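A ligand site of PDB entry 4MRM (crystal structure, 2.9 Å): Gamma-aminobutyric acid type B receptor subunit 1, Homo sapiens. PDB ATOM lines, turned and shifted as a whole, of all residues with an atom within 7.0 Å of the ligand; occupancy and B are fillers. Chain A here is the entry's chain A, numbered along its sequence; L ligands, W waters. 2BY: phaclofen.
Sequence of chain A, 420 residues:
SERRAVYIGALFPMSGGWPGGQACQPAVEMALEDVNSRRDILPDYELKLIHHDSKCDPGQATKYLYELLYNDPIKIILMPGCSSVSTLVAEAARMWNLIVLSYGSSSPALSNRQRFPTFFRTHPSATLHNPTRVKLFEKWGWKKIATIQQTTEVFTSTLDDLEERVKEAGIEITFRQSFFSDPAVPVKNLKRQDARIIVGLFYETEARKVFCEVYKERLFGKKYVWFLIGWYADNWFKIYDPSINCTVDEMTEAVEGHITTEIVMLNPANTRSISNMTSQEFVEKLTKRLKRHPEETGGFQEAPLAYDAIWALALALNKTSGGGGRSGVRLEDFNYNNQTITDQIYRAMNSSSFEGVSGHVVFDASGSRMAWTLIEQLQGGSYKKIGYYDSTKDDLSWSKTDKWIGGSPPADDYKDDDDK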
ATOM      1  N   GLY A  17       1.588 -13.178  -0.847  1.00  0.00           N
ATOM      2  CA  GLY A  17       0.590 -12.779   0.147  1.00  0.00           C
ATOM      3  C   GLY A  17      -0.519 -11.943  -0.441  1.00  0.00           C
ATOM      4  O   GLY A  17      -1.677 -11.997   0.012  1.00  0.00           O
ATOM      5  N   TRP A  18      -0.188 -11.179  -1.479  1.00  0.00           N
ATOM      6  CA  TRP A  18      -1.148 -10.375  -2.188  1.00  0.00           C
ATOM      7  C   TRP A  18      -0.810 -10.434  -3.642  1.00  0.00           C
ATOM      8  O   TRP A  18       0.058  -9.665  -4.082  1.00  0.00           O
ATOM      9  CB  TRP A  18      -1.137  -8.930  -1.654  1.00  0.00           C
ATOM     10  CG  TRP A  18      -2.212  -8.093  -2.254  1.00  0.00           C
ATOM     11  CD1 TRP A  18      -3.558  -8.236  -2.111  1.00  0.00           C
ATOM     12  CD2 TRP A  18      -2.010  -6.963  -3.097  1.00  0.00           C
ATOM     13  NE1 TRP A  18      -4.219  -7.255  -2.796  1.00  0.00           N
ATOM     14  CE2 TRP A  18      -3.295  -6.444  -3.413  1.00  0.00           C
ATOM     15  CE3 TRP A  18      -0.872  -6.313  -3.620  1.00  0.00           C
ATOM     16  CZ2 TRP A  18      -3.488  -5.311  -4.214  1.00  0.00           C
ATOM     17  CZ3 TRP A  18      -1.053  -5.186  -4.414  1.00  0.00           C
ATOM     18  CH2 TRP A  18      -2.356  -4.690  -4.701  1.00  0.00           C
ATOM     19  N   CYS A  56       5.494 -10.531  -4.718  1.00  0.00           N
ATOM     20  CA  CYS A  56       5.245  -9.920  -3.438  1.00  0.00           C
ATOM     21  C   CYS A  56       6.425 -10.244  -2.496  1.00  0.00           C
ATOM     22  O   CYS A  56       6.243 -10.428  -1.266  1.00  0.00           O
ATOM     23  CB  CYS A  56       3.883 -10.323  -2.879  1.00  0.00           C
ATOM     24  SG  CYS A  56       3.259  -9.248  -1.571  1.00  0.00           S
ATOM     25  N   GLY A  81       3.749  -2.473  -5.674  1.00  0.00           N
ATOM     26  CA  GLY A  81       2.446  -2.869  -5.170  1.00  0.00           C
ATOM     27  C   GLY A  81       2.321  -3.252  -3.716  1.00  0.00           C
ATOM     28  O   GLY A  81       1.409  -2.742  -3.040  1.00  0.00           O
ATOM     29  N   CYS A  82       3.156  -4.208  -3.230  1.00  0.00           N
ATOM     30  CA  CYS A  82       3.145  -4.702  -1.835  1.00  0.00           C
ATOM     31  C   CYS A  82       3.735  -3.697  -0.853  1.00  0.00           C
ATOM     32  O   CYS A  82       4.591  -2.915  -1.245  1.00  0.00           O
ATOM     33  CB  CYS A  82       3.824  -6.077  -1.729  1.00  0.00           C
ATOM     34  SG  CYS A  82       2.855  -7.447  -2.413  1.00  0.00           S
ATOM     35  N   SER A  83       3.282  -3.741   0.416  1.00  0.00           N
ATOM     36  CA  SER A  83       3.813  -2.900   1.471  1.00  0.00           C
ATOM     37  C   SER A  83       5.271  -3.290   1.687  1.00  0.00           C
ATOM     38  O   SER A  83       6.136  -2.410   1.763  1.00  0.00           O
ATOM     39  CB  SER A  83       3.013  -3.031   2.747  1.00  0.00           C
ATOM     40  OG  SER A  83       1.874  -2.190   2.752  1.00  0.00           O
ATOM     41  N   SER A  84       5.577  -4.596   1.692  1.00  0.00           N
ATOM     42  CA  SER A  84       6.948  -5.098   1.899  1.00  0.00           C
ATOM     43  C   SER A  84       7.884  -4.692   0.765  1.00  0.00           C
ATOM     44  O   SER A  84       9.049  -4.395   1.009  1.00  0.00           O
ATOM     45  CB  SER A  84       6.978  -6.605   2.132  1.00  0.00           C
ATOM     46  OG  SER A  84       6.547  -7.327   0.993  1.00  0.00           O
ATOM     47  N   VAL A  85       7.368  -4.657  -0.463  1.00  0.00           N
ATOM     48  CA  VAL A  85       8.120  -4.256  -1.644  1.00  0.00           C
ATOM     49  C   VAL A  85       8.269  -2.716  -1.659  1.00  0.00           C
ATOM     50  O   VAL A  85       9.359  -2.220  -1.935  1.00  0.00           O
ATOM     51  CB  VAL A  85       7.514  -4.831  -2.962  1.00  0.00           C
ATOM     52  CG1 VAL A  85       8.143  -4.212  -4.200  1.00  0.00           C
ATOM     53  CG2 VAL A  85       7.646  -6.353  -3.002  1.00  0.00           C
ATOM     54  N   SER A  86       7.193  -1.965  -1.309  1.00  0.00           N
ATOM     55  CA  SER A  86       7.224  -0.502  -1.219  1.00  0.00           C
ATOM     56  C   SER A  86       8.170  -0.022  -0.137  1.00  0.00           C
ATOM     57  O   SER A  86       8.790   1.007  -0.346  1.00  0.00           O
ATOM     58  CB  SER A  86       5.830   0.071  -0.969  1.00  0.00           C
ATOM     59  OG  SER A  86       4.998  -0.004  -2.121  1.00  0.00           O
ATOM     60  N   TYR A 103       0.193   1.599  -5.449  1.00  0.00           N
ATOM     61  CA  TYR A 103      -1.256   1.427  -5.675  1.00  0.00           C
ATOM     62  C   TYR A 103      -1.921   0.444  -4.677  1.00  0.00           C
ATOM     63  O   TYR A 103      -3.148   0.415  -4.596  1.00  0.00           O
ATOM     64  CB  TYR A 103      -1.520   1.006  -7.128  1.00  0.00           C
ATOM     65  CG  TYR A 103      -0.741  -0.216  -7.520  1.00  0.00           C
ATOM     66  CD1 TYR A 103      -1.208  -1.500  -7.227  1.00  0.00           C
ATOM     67  CD2 TYR A 103       0.505  -0.098  -8.127  1.00  0.00           C
ATOM     68  CE1 TYR A 103      -0.445  -2.628  -7.530  1.00  0.00           C
ATOM     69  CE2 TYR A 103       1.274  -1.223  -8.407  1.00  0.00           C
ATOM     70  CZ  TYR A 103       0.788  -2.480  -8.122  1.00  0.00           C
ATOM     71  OH  TYR A 103       1.565  -3.573  -8.392  1.00  0.00           O
ATOM     72  N   GLY A 104      -1.115  -0.352  -3.965  1.00  0.00           N
ATOM     73  CA  GLY A 104      -1.606  -1.373  -3.029  1.00  0.00           C
ATOM     74  C   GLY A 104      -1.042  -1.443  -1.616  1.00  0.00           C
ATOM     75  O   GLY A 104      -1.409  -2.362  -0.887  1.00  0.00           O
ATOM     76  N   SER A 105      -0.173  -0.488  -1.192  1.00  0.00           N
ATOM     77  CA  SER A 105       0.444  -0.488   0.134  1.00  0.00           C
ATOM     78  C   SER A 105      -0.408   0.112   1.241  1.00  0.00           C
ATOM     79  O   SER A 105      -0.757   1.271   1.167  1.00  0.00           O
ATOM     80  CB  SER A 105       1.812   0.181   0.087  1.00  0.00           C
ATOM     81  OG  SER A 105       2.627  -0.520  -0.830  1.00  0.00           O
ATOM     82  N   SER A 106      -0.726  -0.686   2.276  1.00  0.00           N
ATOM     83  CA  SER A 106      -1.539  -0.270   3.417  1.00  0.00           C
ATOM     84  C   SER A 106      -0.767  -0.041   4.740  1.00  0.00           C
ATOM     85  O   SER A 106      -1.338   0.468   5.706  1.00  0.00           O
ATOM     86  CB  SER A 106      -2.668  -1.267   3.649  1.00  0.00           C
ATOM     87  OG  SER A 106      -2.140  -2.533   3.988  1.00  0.00           O
ATOM     88  N   SER A 107       0.535  -0.392   4.768  1.00  0.00           N
ATOM     89  CA  SER A 107       1.421  -0.260   5.932  1.00  0.00           C
ATOM     90  C   SER A 107       1.509   1.174   6.475  1.00  0.00           C
ATOM     91  O   SER A 107       1.970   2.069   5.743  1.00  0.00           O
ATOM     92  CB  SER A 107       2.806  -0.807   5.608  1.00  0.00           C
ATOM     93  OG  SER A 107       3.644  -0.863   6.756  1.00  0.00           O
ATOM     94  N   ARG A 121       1.029   7.059  -2.246  1.00  0.00           N
ATOM     95  CA  ARG A 121       0.276   5.843  -2.478  1.00  0.00           C
ATOM     96  C   ARG A 121      -1.180   6.143  -2.708  1.00  0.00           C
ATOM     97  O   ARG A 121      -1.736   6.992  -1.999  1.00  0.00           O
ATOM     98  CB  ARG A 121       0.449   4.812  -1.373  1.00  0.00           C
ATOM     99  CG  ARG A 121       0.345   5.382   0.034  1.00  0.00           C
ATOM    100  CD  ARG A 121       0.282   4.248   1.030  1.00  0.00           C
ATOM    101  NE  ARG A 121       0.496   4.768   2.371  1.00  0.00           N
ATOM    102  CZ  ARG A 121       0.785   4.003   3.430  1.00  0.00           C
ATOM    103  NH1 ARG A 121       0.870   2.658   3.287  1.00  0.00           N
ATOM    104  NH2 ARG A 121       0.986   4.558   4.633  1.00  0.00           N
ATOM    105  N   HIS A 123      -3.334   3.786  -2.426  1.00  0.00           N
ATOM    106  CA  HIS A 123      -3.906   2.907  -1.435  1.00  0.00           C
ATOM    107  C   HIS A 123      -3.727   3.589  -0.106  1.00  0.00           C
ATOM    108  O   HIS A 123      -2.597   3.966   0.250  1.00  0.00           O
ATOM    109  CB  HIS A 123      -3.141   1.563  -1.398  1.00  0.00           C
ATOM    110  CG  HIS A 123      -3.865   0.492  -0.644  1.00  0.00           C
ATOM    111  ND1 HIS A 123      -4.085   0.592   0.724  1.00  0.00           N
ATOM    112  CD2 HIS A 123      -4.356  -0.697  -1.093  1.00  0.00           C
ATOM    113  CE1 HIS A 123      -4.748  -0.520   1.053  1.00  0.00           C
ATOM    114  NE2 HIS A 123      -4.920  -1.341  -0.008  1.00  0.00           N
ATOM    115  N   VAL A 154       1.579  -4.094  11.640  1.00  0.00           N
ATOM    116  CA  VAL A 154       0.444  -3.318  11.084  1.00  0.00           C
ATOM    117  C   VAL A 154      -0.519  -2.947  12.196  1.00  0.00           C
ATOM    118  O   VAL A 154      -0.955  -1.794  12.271  1.00  0.00           O
ATOM    119  CB  VAL A 154      -0.319  -4.037   9.937  1.00  0.00           C
ATOM    120  CG1 VAL A 154       0.580  -4.320   8.759  1.00  0.00           C
ATOM    121  CG2 VAL A 154      -0.980  -5.339  10.407  1.00  0.00           C
ATOM    122  N   PHE A 155      -0.827  -3.933  13.048  1.00  0.00           N
ATOM    123  CA  PHE A 155      -1.761  -3.789  14.144  1.00  0.00           C
ATOM    124  C   PHE A 155      -1.193  -2.960  15.263  1.00  0.00           C
ATOM    125  O   PHE A 155      -1.935  -2.163  15.843  1.00  0.00           O
ATOM    126  CB  PHE A 155      -2.272  -5.165  14.584  1.00  0.00           C
ATOM    127  CG  PHE A 155      -2.942  -5.916  13.461  1.00  0.00           C
ATOM    128  CD1 PHE A 155      -3.767  -5.252  12.552  1.00  0.00           C
ATOM    129  CD2 PHE A 155      -2.746  -7.286  13.286  1.00  0.00           C
ATOM    130  CE1 PHE A 155      -4.363  -5.937  11.491  1.00  0.00           C
ATOM    131  CE2 PHE A 155      -3.343  -7.970  12.224  1.00  0.00           C
ATOM    132  CZ  PHE A 155      -4.143  -7.296  11.342  1.00  0.00           C
ATOM    133  N   TYR A 203      -5.913 -11.036  11.786  1.00  0.00           N
ATOM    134  CA  TYR A 203      -6.266 -11.616  10.509  1.00  0.00           C
ATOM    135  C   TYR A 203      -7.489 -12.510  10.694  1.00  0.00           C
ATOM    136  O   TYR A 203      -7.983 -12.681  11.825  1.00  0.00           O
ATOM    137  CB  TYR A 203      -5.054 -12.293   9.877  1.00  0.00           C
ATOM    138  CG  TYR A 203      -4.064 -11.255   9.415  1.00  0.00           C
ATOM    139  CD1 TYR A 203      -4.420 -10.284   8.453  1.00  0.00           C
ATOM    140  CD2 TYR A 203      -2.796 -11.162  10.016  1.00  0.00           C
ATOM    141  CE1 TYR A 203      -3.526  -9.284   8.070  1.00  0.00           C
ATOM    142  CE2 TYR A 203      -1.887 -10.171   9.631  1.00  0.00           C
ATOM    143  CZ  TYR A 203      -2.264  -9.231   8.666  1.00  0.00           C
ATOM    144  OH  TYR A 203      -1.391  -8.233   8.289  1.00  0.00           O
ATOM    145  N   TRP A 231     -12.508  -6.274   5.975  1.00  0.00           N
ATOM    146  CA  TRP A 231     -11.949  -7.010   4.850  1.00  0.00           C
ATOM    147  C   TRP A 231     -11.853  -8.526   4.957  1.00  0.00           C
ATOM    148  O   TRP A 231     -11.093  -9.146   4.203  1.00  0.00           O
ATOM    149  CB  TRP A 231     -10.677  -6.378   4.275  1.00  0.00           C
ATOM    150  CG  TRP A 231      -9.600  -5.982   5.256  1.00  0.00           C
ATOM    151  CD1 TRP A 231      -9.103  -4.721   5.439  1.00  0.00           C
ATOM    152  CD2 TRP A 231      -8.765  -6.854   6.028  1.00  0.00           C
ATOM    153  NE1 TRP A 231      -8.039  -4.748   6.311  1.00  0.00           N
ATOM    154  CE2 TRP A 231      -7.808  -6.044   6.693  1.00  0.00           C
ATOM    155  CE3 TRP A 231      -8.756  -8.246   6.266  1.00  0.00           C
ATOM    156  CZ2 TRP A 231      -6.875  -6.561   7.601  1.00  0.00           C
ATOM    157  CZ3 TRP A 231      -7.807  -8.764   7.144  1.00  0.00           C
ATOM    158  CH2 TRP A 231      -6.883  -7.918   7.805  1.00  0.00           C
ATOM    159  N   MET A 265     -13.025   1.730  -2.153  1.00  0.00           N
ATOM    160  CA  MET A 265     -12.071   1.654  -3.264  1.00  0.00           C
ATOM    161  C   MET A 265     -12.693   1.839  -4.637  1.00  0.00           C
ATOM    162  O   MET A 265     -11.983   1.917  -5.638  1.00  0.00           O
ATOM    163  CB  MET A 265     -11.307   0.335  -3.204  1.00  0.00           C
ATOM    164  CG  MET A 265     -10.238   0.342  -2.173  1.00  0.00           C
ATOM    165  SD  MET A 265      -9.520  -1.290  -1.997  1.00  0.00           S
ATOM    166  CE  MET A 265      -8.526  -1.021  -0.608  1.00  0.00           C
ATOM    167  N   GLY A 299      -6.308  -8.717  -6.176  1.00  0.00           N
ATOM    168  CA  GLY A 299      -6.283  -7.265  -6.223  1.00  0.00           C
ATOM    169  C   GLY A 299      -7.318  -6.665  -7.148  1.00  0.00           C
ATOM    170  O   GLY A 299      -7.135  -5.550  -7.639  1.00  0.00           O
ATOM    171  N   GLN A 301     -10.295  -5.605  -6.341  1.00  0.00           N
ATOM    172  CA  GLN A 301     -10.868  -4.455  -5.659  1.00  0.00           C
ATOM    173  C   GLN A 301      -9.884  -3.299  -5.470  1.00  0.00           C
ATOM    174  O   GLN A 301     -10.336  -2.163  -5.253  1.00  0.00           O
ATOM    175  CB  GLN A 301     -11.535  -4.880  -4.355  1.00  0.00           C
ATOM    176  CG  GLN A 301     -10.622  -5.633  -3.395  1.00  0.00           C
ATOM    177  CD  GLN A 301     -10.825  -5.121  -1.981  1.00  0.00           C
ATOM    178  OE1 GLN A 301     -11.813  -4.434  -1.639  1.00  0.00           O
ATOM    179  NE2 GLN A 301      -9.870  -5.447  -1.102  1.00  0.00           N
ATOM    180  N   GLU A 302      -8.560  -3.565  -5.570  1.00  0.00           N
ATOM    181  CA  GLU A 302      -7.544  -2.508  -5.485  1.00  0.00           C
ATOM    182  C   GLU A 302      -7.241  -1.960  -6.879  1.00  0.00           C
ATOM    183  O   GLU A 302      -6.528  -0.955  -7.010  1.00  0.00           O
ATOM    184  CB  GLU A 302      -6.240  -3.036  -4.867  1.00  0.00           C
ATOM    185  CG  GLU A 302      -6.359  -3.339  -3.358  1.00  0.00           C
ATOM    186  CD  GLU A 302      -6.779  -4.774  -3.021  1.00  0.00           C
ATOM    187  OE1 GLU A 302      -6.643  -5.662  -3.910  1.00  0.00           O
ATOM    188  OE2 GLU A 302      -7.225  -4.973  -1.859  1.00  0.00           O
ATOM    189  N   LEU A 305      -7.590   1.798  -7.612  1.00  0.00           N
ATOM    190  CA  LEU A 305      -6.479   2.539  -7.012  1.00  0.00           C
ATOM    191  C   LEU A 305      -5.263   2.560  -7.955  1.00  0.00           C
ATOM    192  O   LEU A 305      -4.608   3.602  -8.077  1.00  0.00           O
ATOM    193  CB  LEU A 305      -6.092   1.988  -5.630  1.00  0.00           C
ATOM    194  CG  LEU A 305      -7.209   1.701  -4.639  1.00  0.00           C
ATOM    195  CD1 LEU A 305      -6.659   0.950  -3.429  1.00  0.00           C
ATOM    196  CD2 LEU A 305      -7.962   2.954  -4.208  1.00  0.00           C
HETATM  197 CL   2BY L   1      -5.067  -8.742   4.638  1.00  0.00          CL
HETATM  198  C3  2BY L   1      -4.406  -7.511   3.516  1.00  0.00           C
HETATM  199  C2  2BY L   1      -3.982  -7.932   2.258  1.00  0.00           C
HETATM  200  C4  2BY L   1      -4.310  -6.175   3.887  1.00  0.00           C
HETATM  201  C5  2BY L   1      -3.781  -5.239   2.972  1.00  0.00           C
HETATM  202  C6  2BY L   1      -3.363  -5.671   1.718  1.00  0.00           C
HETATM  203  C1  2BY L   1      -3.481  -7.010   1.351  1.00  0.00           C
HETATM  204  C7  2BY L   1      -2.792  -4.714   0.759  1.00  0.00           C
HETATM  205  C8  2BY L   1      -3.736  -4.574  -0.443  1.00  0.00           C
HETATM  206  N   2BY L   1      -5.087  -4.269   0.001  1.00  0.00           N
HETATM  207  C9  2BY L   1      -1.452  -5.235   0.255  1.00  0.00           C
HETATM  208  P   2BY L   1      -0.198  -5.195   1.542  1.00  0.00           P
HETATM  209  O1  2BY L   1       1.109  -4.926   0.880  1.00  0.00           O
HETATM  210  O3  2BY L   1      -0.495  -4.030   2.613  1.00  0.00           O
HETATM  211  O2  2BY L   1      -0.085  -6.620   2.286  1.00  0.00           O
HETATM  212  O   HOH W   1      -0.927  -9.215   2.824  1.00  0.00           O
HETATM  213  O   HOH W   2      -1.690  -6.165   5.905  1.00  0.00           O
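Trp 18 touches the ligand (CE2 to C8, 3.5 Å).
Cys 82 touches the ligand (C to O1, 3.4 Å).
Gly 104 touches the ligand (O to C9, 3.1 Å).
CE1 of Tyr 203 touches CL of the ligand, at 3.8 Å.
CZ3 of Trp 231 touches CL of the ligand, at 3.7 Å.
Hydrophobic or aromatic side chains that line the ligand: Trp 18, His 123, Tyr 203 and Trp 231.
Nine residues have an atom within 4 Å of the ligand: Trp 18, Cys 82, Ser 83, Gly 104, Ser 106, His 123, Tyr 203, Trp 231 and Glu 302.
The nearest printed residue that does not touch the ligand is Ser 107 (4.4 Å).
The side-chain hydroxyl (OG) of Ser 83 sits at hydrogen-bond distance from the backbone NH (N) of Ser 106 (3.0 Å).
The side-chain hydroxyl of Ser 83 sits at hydrogen-bond distance from the backbone NH of Ser 107, at 3.0 Å.
The side-chain carboxylate of Glu 302 is in hydrogen-bond range of the indole nitrogen of Trp 18 (3.1 Å).
OE2 of Glu 302 is in hydrogen-bond range of NE2 of Gln 301.
The backbone carbonyl oxygen of Ser 105 lies within hydrogen-bond range of a ring nitrogen (ND1) of His 123 (3.4 Å).
OG of Ser 105 is in hydrogen-bond range of O of Cys 82 (3.1 Å).
The side-chain sulfur (SG) of Cys 82 is disulfide-bonded to the side-chain sulfur (SG) of Cys 56, 2.0 Å away.
The side-chain hydroxyl of Ser 86 sits at hydrogen-bond distance from the backbone carbonyl oxygen of Cys 82.
N of Ser 83 sits at hydrogen-bond distance from O1 of the ligand (2.5 Å).
OG of Ser 83 sits at hydrogen-bond distance from O3 of the ligand (3.0 Å).
O3 of the ligand is in hydrogen-bond range of N of Ser 106 (3.4 Å).
The side-chain hydroxyl (OG) of Ser 106 lies within hydrogen-bond range of an oxygen (O3) of the ligand (2.6 Å).
OE2 of Glu 302 lies within salt-bridge range of N of the ligand (2.9 Å).
NE2 of His 123 sits at hydrogen-bond distance from N of the ligand (2.9 Å).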
